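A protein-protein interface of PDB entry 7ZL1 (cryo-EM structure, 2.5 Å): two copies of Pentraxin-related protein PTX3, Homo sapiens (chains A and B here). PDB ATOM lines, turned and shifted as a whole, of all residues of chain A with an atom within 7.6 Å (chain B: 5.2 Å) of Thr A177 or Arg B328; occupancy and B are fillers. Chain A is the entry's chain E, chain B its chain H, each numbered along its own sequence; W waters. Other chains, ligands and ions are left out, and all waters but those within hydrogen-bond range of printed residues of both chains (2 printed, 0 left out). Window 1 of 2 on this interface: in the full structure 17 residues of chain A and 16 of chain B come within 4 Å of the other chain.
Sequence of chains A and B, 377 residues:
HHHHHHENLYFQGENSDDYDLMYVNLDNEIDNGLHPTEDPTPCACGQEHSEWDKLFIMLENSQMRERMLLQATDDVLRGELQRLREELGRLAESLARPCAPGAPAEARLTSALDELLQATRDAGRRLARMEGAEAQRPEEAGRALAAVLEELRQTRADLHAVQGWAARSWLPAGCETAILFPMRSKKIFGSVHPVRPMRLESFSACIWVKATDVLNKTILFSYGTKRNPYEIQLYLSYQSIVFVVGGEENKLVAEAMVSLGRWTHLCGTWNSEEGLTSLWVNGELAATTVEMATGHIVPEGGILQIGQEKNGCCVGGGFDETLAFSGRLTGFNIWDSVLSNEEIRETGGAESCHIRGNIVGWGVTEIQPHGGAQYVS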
ATOM      1  N   LEU A 171      11.781  15.938 -20.938  1.00  0.00           N
ATOM      2  CA  LEU A 171      12.433  16.528 -22.093  1.00  0.00           C
ATOM      3  C   LEU A 171      12.132  15.710 -23.340  1.00  0.00           C
ATOM      4  O   LEU A 171      12.042  14.484 -23.274  1.00  0.00           O
ATOM      5  CB  LEU A 171      13.949  16.636 -21.906  1.00  0.00           C
ATOM      6  CG  LEU A 171      14.455  17.677 -20.907  1.00  0.00           C
ATOM      7  CD1 LEU A 171      15.952  17.696 -20.901  1.00  0.00           C
ATOM      8  CD2 LEU A 171      13.933  19.069 -21.247  1.00  0.00           C
ATOM      9  N   PRO A 172      11.995  16.359 -24.492  1.00  0.00           N
ATOM     10  CA  PRO A 172      11.291  15.727 -25.614  1.00  0.00           C
ATOM     11  C   PRO A 172      11.893  14.445 -26.166  1.00  0.00           C
ATOM     12  O   PRO A 172      11.337  13.368 -25.936  1.00  0.00           O
ATOM     13  CB  PRO A 172      11.282  16.831 -26.679  1.00  0.00           C
ATOM     14  CG  PRO A 172      12.293  17.813 -26.242  1.00  0.00           C
ATOM     15  CD  PRO A 172      12.280  17.773 -24.764  1.00  0.00           C
ATOM     16  N   GLY A 174      15.363  11.820 -26.569  1.00  0.00           N
ATOM     17  CA  GLY A 174      16.204  11.348 -25.487  1.00  0.00           C
ATOM     18  C   GLY A 174      17.036  12.429 -24.819  1.00  0.00           C
ATOM     19  O   GLY A 174      18.006  12.109 -24.130  1.00  0.00           O
ATOM     20  N   CYS A 175      16.685  13.701 -25.003  1.00  0.00           N
ATOM     21  CA  CYS A 175      17.549  14.797 -24.579  1.00  0.00           C
ATOM     22  C   CYS A 175      17.698  14.857 -23.071  1.00  0.00           C
ATOM     23  O   CYS A 175      16.731  14.725 -22.319  1.00  0.00           O
ATOM     24  CB  CYS A 175      17.054  16.141 -25.112  1.00  0.00           C
ATOM     25  SG  CYS A 175      17.218  16.310 -26.916  1.00  0.00           S
ATOM     26  N   GLU A 176      18.939  15.026 -22.647  1.00  0.00           N
ATOM     27  CA  GLU A 176      19.346  14.890 -21.264  1.00  0.00           C
ATOM     28  C   GLU A 176      19.834  16.232 -20.724  1.00  0.00           C
ATOM     29  O   GLU A 176      20.455  16.274 -19.660  1.00  0.00           O
ATOM     30  CB  GLU A 176      20.401  13.781 -21.201  1.00  0.00           C
ATOM     31  CG  GLU A 176      20.634  13.146 -19.860  1.00  0.00           C
ATOM     32  CD  GLU A 176      21.447  11.866 -19.979  1.00  0.00           C
ATOM     33  OE1 GLU A 176      21.023  10.966 -20.735  1.00  0.00           O
ATOM     34  OE2 GLU A 176      22.480  11.730 -19.292  1.00  0.00           O
ATOM     35  N   THR A 177      19.573  17.321 -21.457  1.00  0.00           N
ATOM     36  CA  THR A 177      20.008  18.687 -21.175  1.00  0.00           C
ATOM     37  C   THR A 177      19.088  19.652 -21.921  1.00  0.00           C
ATOM     38  O   THR A 177      18.702  19.386 -23.055  1.00  0.00           O
ATOM     39  CB  THR A 177      21.466  18.912 -21.618  1.00  0.00           C
ATOM     40  OG1 THR A 177      22.342  18.027 -20.911  1.00  0.00           O
ATOM     41  CG2 THR A 177      21.905  20.345 -21.400  1.00  0.00           C
ATOM     42  N   ALA A 178      18.757  20.775 -21.293  1.00  0.00           N
ATOM     43  CA  ALA A 178      18.046  21.858 -21.958  1.00  0.00           C
ATOM     44  C   ALA A 178      18.587  23.191 -21.460  1.00  0.00           C
ATOM     45  O   ALA A 178      19.384  23.247 -20.525  1.00  0.00           O
ATOM     46  CB  ALA A 178      16.535  21.751 -21.728  1.00  0.00           C
ATOM     47  N   ILE A 179      18.172  24.275 -22.107  1.00  0.00           N
ATOM     48  CA  ILE A 179      18.435  25.630 -21.639  1.00  0.00           C
ATOM     49  C   ILE A 179      17.116  26.293 -21.276  1.00  0.00           C
ATOM     50  O   ILE A 179      16.208  26.378 -22.107  1.00  0.00           O
ATOM     51  CB  ILE A 179      19.199  26.448 -22.693  1.00  0.00           C
ATOM     52  CG1 ILE A 179      20.573  25.827 -22.939  1.00  0.00           C
ATOM     53  CG2 ILE A 179      19.356  27.886 -22.248  1.00  0.00           C
ATOM     54  CD1 ILE A 179      21.241  26.310 -24.192  1.00  0.00           C
ATOM     55  N   TRP A 263       6.229  21.078 -25.806  1.00  0.00           N
ATOM     56  CA  TRP A 263       7.428  20.802 -26.586  1.00  0.00           C
ATOM     57  C   TRP A 263       7.070  20.538 -28.038  1.00  0.00           C
ATOM     58  O   TRP A 263       6.341  19.596 -28.348  1.00  0.00           O
ATOM     59  CB  TRP A 263       8.176  19.607 -26.007  1.00  0.00           C
ATOM     60  CG  TRP A 263       9.004  19.922 -24.809  1.00  0.00           C
ATOM     61  CD1 TRP A 263       8.764  19.528 -23.537  1.00  0.00           C
ATOM     62  CD2 TRP A 263      10.212  20.686 -24.771  1.00  0.00           C
ATOM     63  NE1 TRP A 263       9.746  19.987 -22.703  1.00  0.00           N
ATOM     64  CE2 TRP A 263      10.644  20.712 -23.434  1.00  0.00           C
ATOM     65  CE3 TRP A 263      10.973  21.347 -25.736  1.00  0.00           C
ATOM     66  CZ2 TRP A 263      11.798  21.371 -23.037  1.00  0.00           C
ATOM     67  CZ3 TRP A 263      12.117  22.001 -25.337  1.00  0.00           C
ATOM     68  CH2 TRP A 263      12.518  22.012 -24.001  1.00  0.00           C
ATOM     69  N   LEU A 329      14.650  25.507 -24.356  1.00  0.00           N
ATOM     70  CA  LEU A 329      15.165  25.067 -25.646  1.00  0.00           C
ATOM     71  C   LEU A 329      16.055  23.847 -25.463  1.00  0.00           C
ATOM     72  O   LEU A 329      16.747  23.712 -24.456  1.00  0.00           O
ATOM     73  CB  LEU A 329      15.976  26.163 -26.337  1.00  0.00           C
ATOM     74  CG  LEU A 329      15.279  27.484 -26.628  1.00  0.00           C
ATOM     75  CD1 LEU A 329      16.287  28.496 -27.112  1.00  0.00           C
ATOM     76  CD2 LEU A 329      14.164  27.312 -27.650  1.00  0.00           C
ATOM     77  N   THR A 330      16.019  22.945 -26.433  1.00  0.00           N
ATOM     78  CA  THR A 330      16.980  21.855 -26.475  1.00  0.00           C
ATOM     79  C   THR A 330      17.168  21.430 -27.925  1.00  0.00           C
ATOM     80  O   THR A 330      16.416  21.830 -28.807  1.00  0.00           O
ATOM     81  CB  THR A 330      16.533  20.691 -25.579  1.00  0.00           C
ATOM     82  OG1 THR A 330      17.594  19.746 -25.457  1.00  0.00           O
ATOM     83  CG2 THR A 330      15.313  19.996 -26.141  1.00  0.00           C
ATOM     84  N   GLY A 331      18.203  20.636 -28.163  1.00  0.00           N
ATOM     85  CA  GLY A 331      18.399  20.012 -29.459  1.00  0.00           C
ATOM     86  C   GLY A 331      18.583  20.959 -30.622  1.00  0.00           C
ATOM     87  O   GLY A 331      18.137  20.657 -31.727  1.00  0.00           O
ATOM     88  N   CYS A 353      17.550  12.474 -30.047  1.00  0.00           N
ATOM     89  CA  CYS A 353      18.456  13.509 -29.544  1.00  0.00           C
ATOM     90  C   CYS A 353      19.918  13.232 -29.878  1.00  0.00           C
ATOM     91  O   CYS A 353      20.716  14.170 -29.917  1.00  0.00           O
ATOM     92  CB  CYS A 353      18.307  13.671 -28.031  1.00  0.00           C
ATOM     93  SG  CYS A 353      18.912  15.273 -27.396  1.00  0.00           S
ATOM     94  N   TRP A 362      23.988  19.760 -30.977  1.00  0.00           N
ATOM     95  CA  TRP A 362      23.608  19.879 -29.580  1.00  0.00           C
ATOM     96  C   TRP A 362      24.436  18.926 -28.728  1.00  0.00           C
ATOM     97  O   TRP A 362      24.525  17.732 -29.017  1.00  0.00           O
ATOM     98  CB  TRP A 362      22.120  19.589 -29.418  1.00  0.00           C
ATOM     99  CG  TRP A 362      21.619  19.852 -28.045  1.00  0.00           C
ATOM    100  CD1 TRP A 362      21.275  18.924 -27.113  1.00  0.00           C
ATOM    101  CD2 TRP A 362      21.407  21.127 -27.439  1.00  0.00           C
ATOM    102  NE1 TRP A 362      20.858  19.541 -25.968  1.00  0.00           N
ATOM    103  CE2 TRP A 362      20.935  20.895 -26.139  1.00  0.00           C
ATOM    104  CE3 TRP A 362      21.567  22.443 -27.871  1.00  0.00           C
ATOM    105  CZ2 TRP A 362      20.615  21.926 -25.270  1.00  0.00           C
ATOM    106  CZ3 TRP A 362      21.258  23.453 -27.014  1.00  0.00           C
ATOM    107  CH2 TRP A 362      20.793  23.194 -25.719  1.00  0.00           C
ATOM    108  N   GLY A 363      25.030  19.451 -27.664  1.00  0.00           N
ATOM    109  CA  GLY A 363      25.923  18.687 -26.825  1.00  0.00           C
ATOM    110  C   GLY A 363      27.378  18.639 -27.245  1.00  0.00           C
ATOM    111  O   GLY A 363      28.189  18.080 -26.504  1.00  0.00           O
ATOM    112  N   GLN A 374      19.911  29.465 -18.230  1.00  0.00           N
ATOM    113  CA  GLN A 374      20.511  28.397 -17.441  1.00  0.00           C
ATOM    114  C   GLN A 374      20.462  27.095 -18.219  1.00  0.00           C
ATOM    115  O   GLN A 374      19.455  26.793 -18.857  1.00  0.00           O
ATOM    116  CB  GLN A 374      19.774  28.172 -16.125  1.00  0.00           C
ATOM    117  CG  GLN A 374      19.540  29.384 -15.290  1.00  0.00           C
ATOM    118  CD  GLN A 374      18.557  29.103 -14.175  1.00  0.00           C
ATOM    119  OE1 GLN A 374      18.416  27.963 -13.735  1.00  0.00           O
ATOM    120  NE2 GLN A 374      17.838  30.131 -13.745  1.00  0.00           N
ATOM    121  N   TYR A 375      21.532  26.316 -18.147  1.00  0.00           N
ATOM    122  CA  TYR A 375      21.418  24.891 -18.427  1.00  0.00           C
ATOM    123  C   TYR A 375      20.561  24.222 -17.370  1.00  0.00           C
ATOM    124  O   TYR A 375      20.742  24.451 -16.175  1.00  0.00           O
ATOM    125  CB  TYR A 375      22.787  24.232 -18.483  1.00  0.00           C
ATOM    126  CG  TYR A 375      23.424  24.287 -19.841  1.00  0.00           C
ATOM    127  CD1 TYR A 375      22.882  23.588 -20.903  1.00  0.00           C
ATOM    128  CD2 TYR A 375      24.584  25.007 -20.056  1.00  0.00           C
ATOM    129  CE1 TYR A 375      23.459  23.629 -22.150  1.00  0.00           C
ATOM    130  CE2 TYR A 375      25.168  25.055 -21.296  1.00  0.00           C
ATOM    131  CZ  TYR A 375      24.603  24.366 -22.342  1.00  0.00           C
ATOM    132  OH  TYR A 375      25.197  24.401 -23.574  1.00  0.00           O
ATOM    133  N   VAL A 376      19.606  23.408 -17.810  1.00  0.00           N
ATOM    134  CA  VAL A 376      18.702  22.794 -16.849  1.00  0.00           C
ATOM    135  C   VAL A 376      19.355  21.587 -16.192  1.00  0.00           C
ATOM    136  O   VAL A 376      19.019  21.245 -15.052  1.00  0.00           O
ATOM    137  CB  VAL A 376      17.360  22.423 -17.498  1.00  0.00           C
ATOM    138  CG1 VAL A 376      16.377  22.025 -16.435  1.00  0.00           C
ATOM    139  CG2 VAL A 376      16.803  23.586 -18.297  1.00  0.00           C
ATOM    140  N   SER A 377      20.283  20.921 -16.869  1.00  0.00           N
ATOM    141  CA  SER A 377      21.135  19.947 -16.188  1.00  0.00           C
ATOM    142  C   SER A 377      21.917  20.639 -15.077  1.00  0.00           C
ATOM    143  O   SER A 377      22.696  20.005 -14.365  1.00  0.00           O
ATOM    144  CB  SER A 377      22.105  19.268 -17.155  1.00  0.00           C
ATOM    145  OG  SER A 377      21.432  18.686 -18.251  1.00  0.00           O
ATOM    146  N   ALA B 178      27.875  13.263 -10.509  1.00  0.00           N
ATOM    147  CA  ALA B 178      28.646  13.132 -11.729  1.00  0.00           C
ATOM    148  C   ALA B 178      29.118  14.512 -12.148  1.00  0.00           C
ATOM    149  O   ALA B 178      28.692  15.529 -11.603  1.00  0.00           O
ATOM    150  CB  ALA B 178      27.835  12.463 -12.843  1.00  0.00           C
ATOM    151  N   ILE B 179      30.036  14.546 -13.102  1.00  0.00           N
ATOM    152  CA  ILE B 179      30.435  15.778 -13.762  1.00  0.00           C
ATOM    153  C   ILE B 179      29.923  15.741 -15.192  1.00  0.00           C
ATOM    154  O   ILE B 179      30.220  14.806 -15.939  1.00  0.00           O
ATOM    155  CB  ILE B 179      31.959  15.967 -13.706  1.00  0.00           C
ATOM    156  CG1 ILE B 179      32.402  16.103 -12.250  1.00  0.00           C
ATOM    157  CG2 ILE B 179      32.372  17.188 -14.495  1.00  0.00           C
ATOM    158  CD1 ILE B 179      33.882  15.978 -12.046  1.00  0.00           C
ATOM    159  N   LEU B 180      29.177  16.769 -15.575  1.00  0.00           N
ATOM    160  CA  LEU B 180      28.690  16.939 -16.936  1.00  0.00           C
ATOM    161  C   LEU B 180      29.636  17.835 -17.722  1.00  0.00           C
ATOM    162  O   LEU B 180      30.045  18.888 -17.234  1.00  0.00           O
ATOM    163  CB  LEU B 180      27.280  17.530 -16.927  1.00  0.00           C
ATOM    164  CG  LEU B 180      26.734  18.090 -18.242  1.00  0.00           C
ATOM    165  CD1 LEU B 180      26.562  17.009 -19.281  1.00  0.00           C
ATOM    166  CD2 LEU B 180      25.432  18.806 -17.999  1.00  0.00           C
ATOM    167  N   PHE B 181      30.009  17.389 -18.919  1.00  0.00           N
ATOM    168  CA  PHE B 181      30.652  18.220 -19.926  1.00  0.00           C
ATOM    169  C   PHE B 181      29.640  18.562 -21.003  1.00  0.00           C
ATOM    170  O   PHE B 181      29.461  17.778 -21.941  1.00  0.00           O
ATOM    171  CB  PHE B 181      31.852  17.495 -20.531  1.00  0.00           C
ATOM    172  CG  PHE B 181      33.058  17.494 -19.659  1.00  0.00           C
ATOM    173  CD1 PHE B 181      33.046  16.863 -18.431  1.00  0.00           C
ATOM    174  CD2 PHE B 181      34.221  18.104 -20.077  1.00  0.00           C
ATOM    175  CE1 PHE B 181      34.163  16.861 -17.645  1.00  0.00           C
ATOM    176  CE2 PHE B 181      35.337  18.100 -19.285  1.00  0.00           C
ATOM    177  CZ  PHE B 181      35.306  17.482 -18.070  1.00  0.00           C
ATOM    178  N   TRP B 208      33.999   5.813 -14.738  1.00  0.00           N
ATOM    179  CA  TRP B 208      32.750   5.659 -15.474  1.00  0.00           C
ATOM    180  C   TRP B 208      32.625   6.780 -16.494  1.00  0.00           C
ATOM    181  O   TRP B 208      32.736   7.955 -16.142  1.00  0.00           O
ATOM    182  CB  TRP B 208      31.549   5.703 -14.527  1.00  0.00           C
ATOM    183  CG  TRP B 208      31.327   4.476 -13.712  1.00  0.00           C
ATOM    184  CD1 TRP B 208      31.722   4.266 -12.430  1.00  0.00           C
ATOM    185  CD2 TRP B 208      30.625   3.301 -14.113  1.00  0.00           C
ATOM    186  NE1 TRP B 208      31.322   3.032 -12.009  1.00  0.00           N
ATOM    187  CE2 TRP B 208      30.646   2.415 -13.026  1.00  0.00           C
ATOM    188  CE3 TRP B 208      29.985   2.908 -15.287  1.00  0.00           C
ATOM    189  CZ2 TRP B 208      30.053   1.161 -13.078  1.00  0.00           C
ATOM    190  CZ3 TRP B 208      29.399   1.667 -15.335  1.00  0.00           C
ATOM    191  CH2 TRP B 208      29.439   0.807 -14.243  1.00  0.00           C
ATOM    192  N   VAL B 209      32.352   6.427 -17.741  1.00  0.00           N
ATOM    193  CA  VAL B 209      32.202   7.408 -18.803  1.00  0.00           C
ATOM    194  C   VAL B 209      30.876   7.197 -19.516  1.00  0.00           C
ATOM    195  O   VAL B 209      30.457   6.064 -19.762  1.00  0.00           O
ATOM    196  CB  VAL B 209      33.383   7.351 -19.795  1.00  0.00           C
ATOM    197  CG1 VAL B 209      33.475   6.000 -20.452  1.00  0.00           C
ATOM    198  CG2 VAL B 209      33.236   8.438 -20.836  1.00  0.00           C
ATOM    199  N   LYS B 210      30.218   8.296 -19.853  1.00  0.00           N
ATOM    200  CA  LYS B 210      29.076   8.293 -20.760  1.00  0.00           C
ATOM    201  C   LYS B 210      29.366   9.314 -21.853  1.00  0.00           C
ATOM    202  O   LYS B 210      28.966  10.471 -21.758  1.00  0.00           O
ATOM    203  CB  LYS B 210      27.814   8.593 -20.019  1.00  0.00           C
ATOM    204  CG  LYS B 210      26.575   8.390 -20.831  1.00  0.00           C
ATOM    205  CD  LYS B 210      25.386   8.824 -20.050  1.00  0.00           C
ATOM    206  CE  LYS B 210      24.103   8.501 -20.745  1.00  0.00           C
ATOM    207  NZ  LYS B 210      22.951   8.931 -19.936  1.00  0.00           N
ATOM    208  N   ALA B 211      30.072   8.880 -22.887  1.00  0.00           N
ATOM    209  CA  ALA B 211      30.505   9.785 -23.939  1.00  0.00           C
ATOM    210  C   ALA B 211      29.341  10.227 -24.814  1.00  0.00           C
ATOM    211  O   ALA B 211      28.541   9.408 -25.264  1.00  0.00           O
ATOM    212  CB  ALA B 211      31.574   9.118 -24.793  1.00  0.00           C
ATOM    213  N   TRP B 263      26.450   4.359 -20.208  1.00  0.00           N
ATOM    214  CA  TRP B 263      27.415   4.304 -19.111  1.00  0.00           C
ATOM    215  C   TRP B 263      28.248   3.036 -19.191  1.00  0.00           C
ATOM    216  O   TRP B 263      27.723   1.927 -19.086  1.00  0.00           O
ATOM    217  CB  TRP B 263      26.685   4.357 -17.767  1.00  0.00           C
ATOM    218  CG  TRP B 263      26.268   5.716 -17.285  1.00  0.00           C
ATOM    219  CD1 TRP B 263      24.999   6.156 -17.124  1.00  0.00           C
ATOM    220  CD2 TRP B 263      27.119   6.789 -16.859  1.00  0.00           C
ATOM    221  NE1 TRP B 263      24.994   7.448 -16.675  1.00  0.00           N
ATOM    222  CE2 TRP B 263      26.284   7.849 -16.466  1.00  0.00           C
ATOM    223  CE3 TRP B 263      28.501   6.954 -16.758  1.00  0.00           C
ATOM    224  CZ2 TRP B 263      26.784   9.057 -15.998  1.00  0.00           C
ATOM    225  CZ3 TRP B 263      28.992   8.161 -16.309  1.00  0.00           C
ATOM    226  CH2 TRP B 263      28.138   9.193 -15.926  1.00  0.00           C
ATOM    227  N   PHE B 325      36.678  16.078 -23.935  1.00  0.00           N
ATOM    228  CA  PHE B 325      35.547  15.209 -23.668  1.00  0.00           C
ATOM    229  C   PHE B 325      34.235  15.983 -23.689  1.00  0.00           C
ATOM    230  O   PHE B 325      34.171  17.153 -23.311  1.00  0.00           O
ATOM    231  CB  PHE B 325      35.737  14.538 -22.308  1.00  0.00           C
ATOM    232  CG  PHE B 325      34.654  13.585 -21.940  1.00  0.00           C
ATOM    233  CD1 PHE B 325      34.493  12.403 -22.623  1.00  0.00           C
ATOM    234  CD2 PHE B 325      33.796  13.873 -20.898  1.00  0.00           C
ATOM    235  CE1 PHE B 325      33.503  11.529 -22.277  1.00  0.00           C
ATOM    236  CE2 PHE B 325      32.799  12.996 -20.550  1.00  0.00           C
ATOM    237  CZ  PHE B 325      32.652  11.824 -21.244  1.00  0.00           C
ATOM    238  N   SER B 326      33.175  15.309 -24.103  1.00  0.00           N
ATOM    239  CA  SER B 326      31.819  15.763 -23.840  1.00  0.00           C
ATOM    240  C   SER B 326      30.966  14.566 -23.450  1.00  0.00           C
ATOM    241  O   SER B 326      31.123  13.477 -23.999  1.00  0.00           O
ATOM    242  CB  SER B 326      31.234  16.510 -25.046  1.00  0.00           C
ATOM    243  OG  SER B 326      31.103  15.673 -26.172  1.00  0.00           O
ATOM    244  N   GLY B 327      30.052  14.788 -22.514  1.00  0.00           N
ATOM    245  CA  GLY B 327      29.315  13.721 -21.875  1.00  0.00           C
ATOM    246  C   GLY B 327      29.362  13.842 -20.370  1.00  0.00           C
ATOM    247  O   GLY B 327      29.478  14.949 -19.847  1.00  0.00           O
ATOM    248  N   ARG B 328      29.247  12.720 -19.666  1.00  0.00           N
ATOM    249  CA  ARG B 328      29.251  12.683 -18.212  1.00  0.00           C
ATOM    250  C   ARG B 328      30.330  11.735 -17.705  1.00  0.00           C
ATOM    251  O   ARG B 328      30.638  10.725 -18.337  1.00  0.00           O
ATOM    252  CB  ARG B 328      27.884  12.259 -17.662  1.00  0.00           C
ATOM    253  CG  ARG B 328      26.784  13.267 -17.939  1.00  0.00           C
ATOM    254  CD  ARG B 328      25.394  12.722 -17.664  1.00  0.00           C
ATOM    255  NE  ARG B 328      24.429  13.795 -17.448  1.00  0.00           N
ATOM    256  CZ  ARG B 328      23.869  14.510 -18.413  1.00  0.00           C
ATOM    257  NH1 ARG B 328      24.175  14.318 -19.684  1.00  0.00           N
ATOM    258  NH2 ARG B 328      23.016  15.477 -18.092  1.00  0.00           N
ATOM    259  N   LEU B 329      30.899  12.073 -16.551  1.00  0.00           N
ATOM    260  CA  LEU B 329      31.908  11.263 -15.880  1.00  0.00           C
ATOM    261  C   LEU B 329      31.552  11.098 -14.411  1.00  0.00           C
ATOM    262  O   LEU B 329      30.990  12.004 -13.796  1.00  0.00           O
ATOM    263  CB  LEU B 329      33.295  11.896 -15.977  1.00  0.00           C
ATOM    264  CG  LEU B 329      33.888  12.122 -17.360  1.00  0.00           C
ATOM    265  CD1 LEU B 329      35.166  12.913 -17.242  1.00  0.00           C
ATOM    266  CD2 LEU B 329      34.140  10.807 -18.082  1.00  0.00           C
ATOM    267  N   THR B 330      31.856   9.934 -13.858  1.00  0.00           N
ATOM    268  CA  THR B 330      31.739   9.732 -12.423  1.00  0.00           C
ATOM    269  C   THR B 330      32.722   8.646 -12.010  1.00  0.00           C
ATOM    270  O   THR B 330      33.286   7.947 -12.844  1.00  0.00           O
ATOM    271  CB  THR B 330      30.296   9.393 -12.027  1.00  0.00           C
ATOM    272  OG1 THR B 330      30.173   9.406 -10.606  1.00  0.00           O
ATOM    273  CG2 THR B 330      29.888   8.034 -12.544  1.00  0.00           C
ATOM    274  N   VAL B 376      26.663  17.788 -11.460  1.00  0.00           N
ATOM    275  CA  VAL B 376      25.225  17.661 -11.642  1.00  0.00           C
ATOM    276  C   VAL B 376      24.565  17.012 -10.431  1.00  0.00           C
ATOM    277  O   VAL B 376      23.401  16.609 -10.499  1.00  0.00           O
ATOM    278  CB  VAL B 376      24.873  16.950 -12.960  1.00  0.00           C
ATOM    279  CG1 VAL B 376      25.365  17.796 -14.124  1.00  0.00           C
ATOM    280  CG2 VAL B 376      25.477  15.577 -13.028  1.00  0.00           C
HETATM  281  O   HOH W   1      23.175  10.410 -16.459  1.00  0.00           O
HETATM  282  O   HOH W   2      27.544  16.801 -24.188  1.00  0.00           O
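The side-chain carboxylate (OE2) of Glu A176 lies within salt-bridge range of the side-chain amino group (NZ) of Lys B210 (2.9 Å).
OE2 of Glu A176 is in salt-bridge range of NH1 of Arg B328 (3.1 Å).
O of Glu A176 sits at hydrogen-bond distance from OG of Ser A377.
O of Thr A177 sits at hydrogen-bond distance from OG1 of Thr A330, 2.7 Å away.
The side-chain hydroxyl of Thr A177 lies within hydrogen-bond range of the side-chain hydroxyl of Ser A377 (2.9 Å).
The backbone NH (N) of Val B376 sits at hydrogen-bond distance from the backbone carbonyl oxygen (O) of Ala B178, at 3.0 Å.
O of Arg B328 is in hydrogen-bond range of N of Lys B210 (2.9 Å).
SG of Cys A353 forms a disulfide with SG of Cys A175, at 2.0 Å.
Among the printed residues, merely in contact across the chains: Ser A377 with Leu B180 (3.5 Å), Ser A377 with Val B376 (3.5 Å), Ser A377 with Arg B328 (3.6 Å), Gly A363 with Ser B326 (3.7 Å) and Thr A177 with Arg B328 (3.9 Å).
Of the printed residues of chain B, Glu A176 touches Lys B210 and Arg B328.
Of chain B, only Arg B328 comes within 4 Å of Thr A177.
Printed residues of chain B within 4 Å of Ser A377: Leu B180, Arg B328 and Val B376.
Of the printed residues of chain A, Leu B180 touches Ser A377 (3.5 Å).
Phe B181 touches none of the printed residues of chain A.
The nearest residue of chain B that does not touch Thr A177 is Leu B180 (4.3 Å).
The nearest residue of chain A that does not touch Arg B328 is Cys A175 (7.3 Å).
The nearest printed residue of chain B that does not touch Gly A363 is Phe B181 (4.7 Å).
Of the 16 printed residues of chain B, 5 touch a printed residue of chain A.
Hydrophobic or aromatic side chains of chain B within 4 Å of the printed part of chain A: Leu B180 and Val B376.
Of the 19 printed residues of chain A, 4 touch a printed residue of chain B.
Among the printed residues, Asp or Glu carboxylates within 4 Å of a Lys or Arg side-chain nitrogen of the other chain: Glu A176 with Lys B210 (2.9 Å) and Glu A176 with Arg B328 (3.1 Å).
6 positions are printed for both chains.
Water W2 bridges O of Gly A363 and O of Phe B181.
Water W1 lies within hydrogen-bond range of OE2 of Glu A176 (3.2 Å) and NE1 of Trp B263 (3.5 Å).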
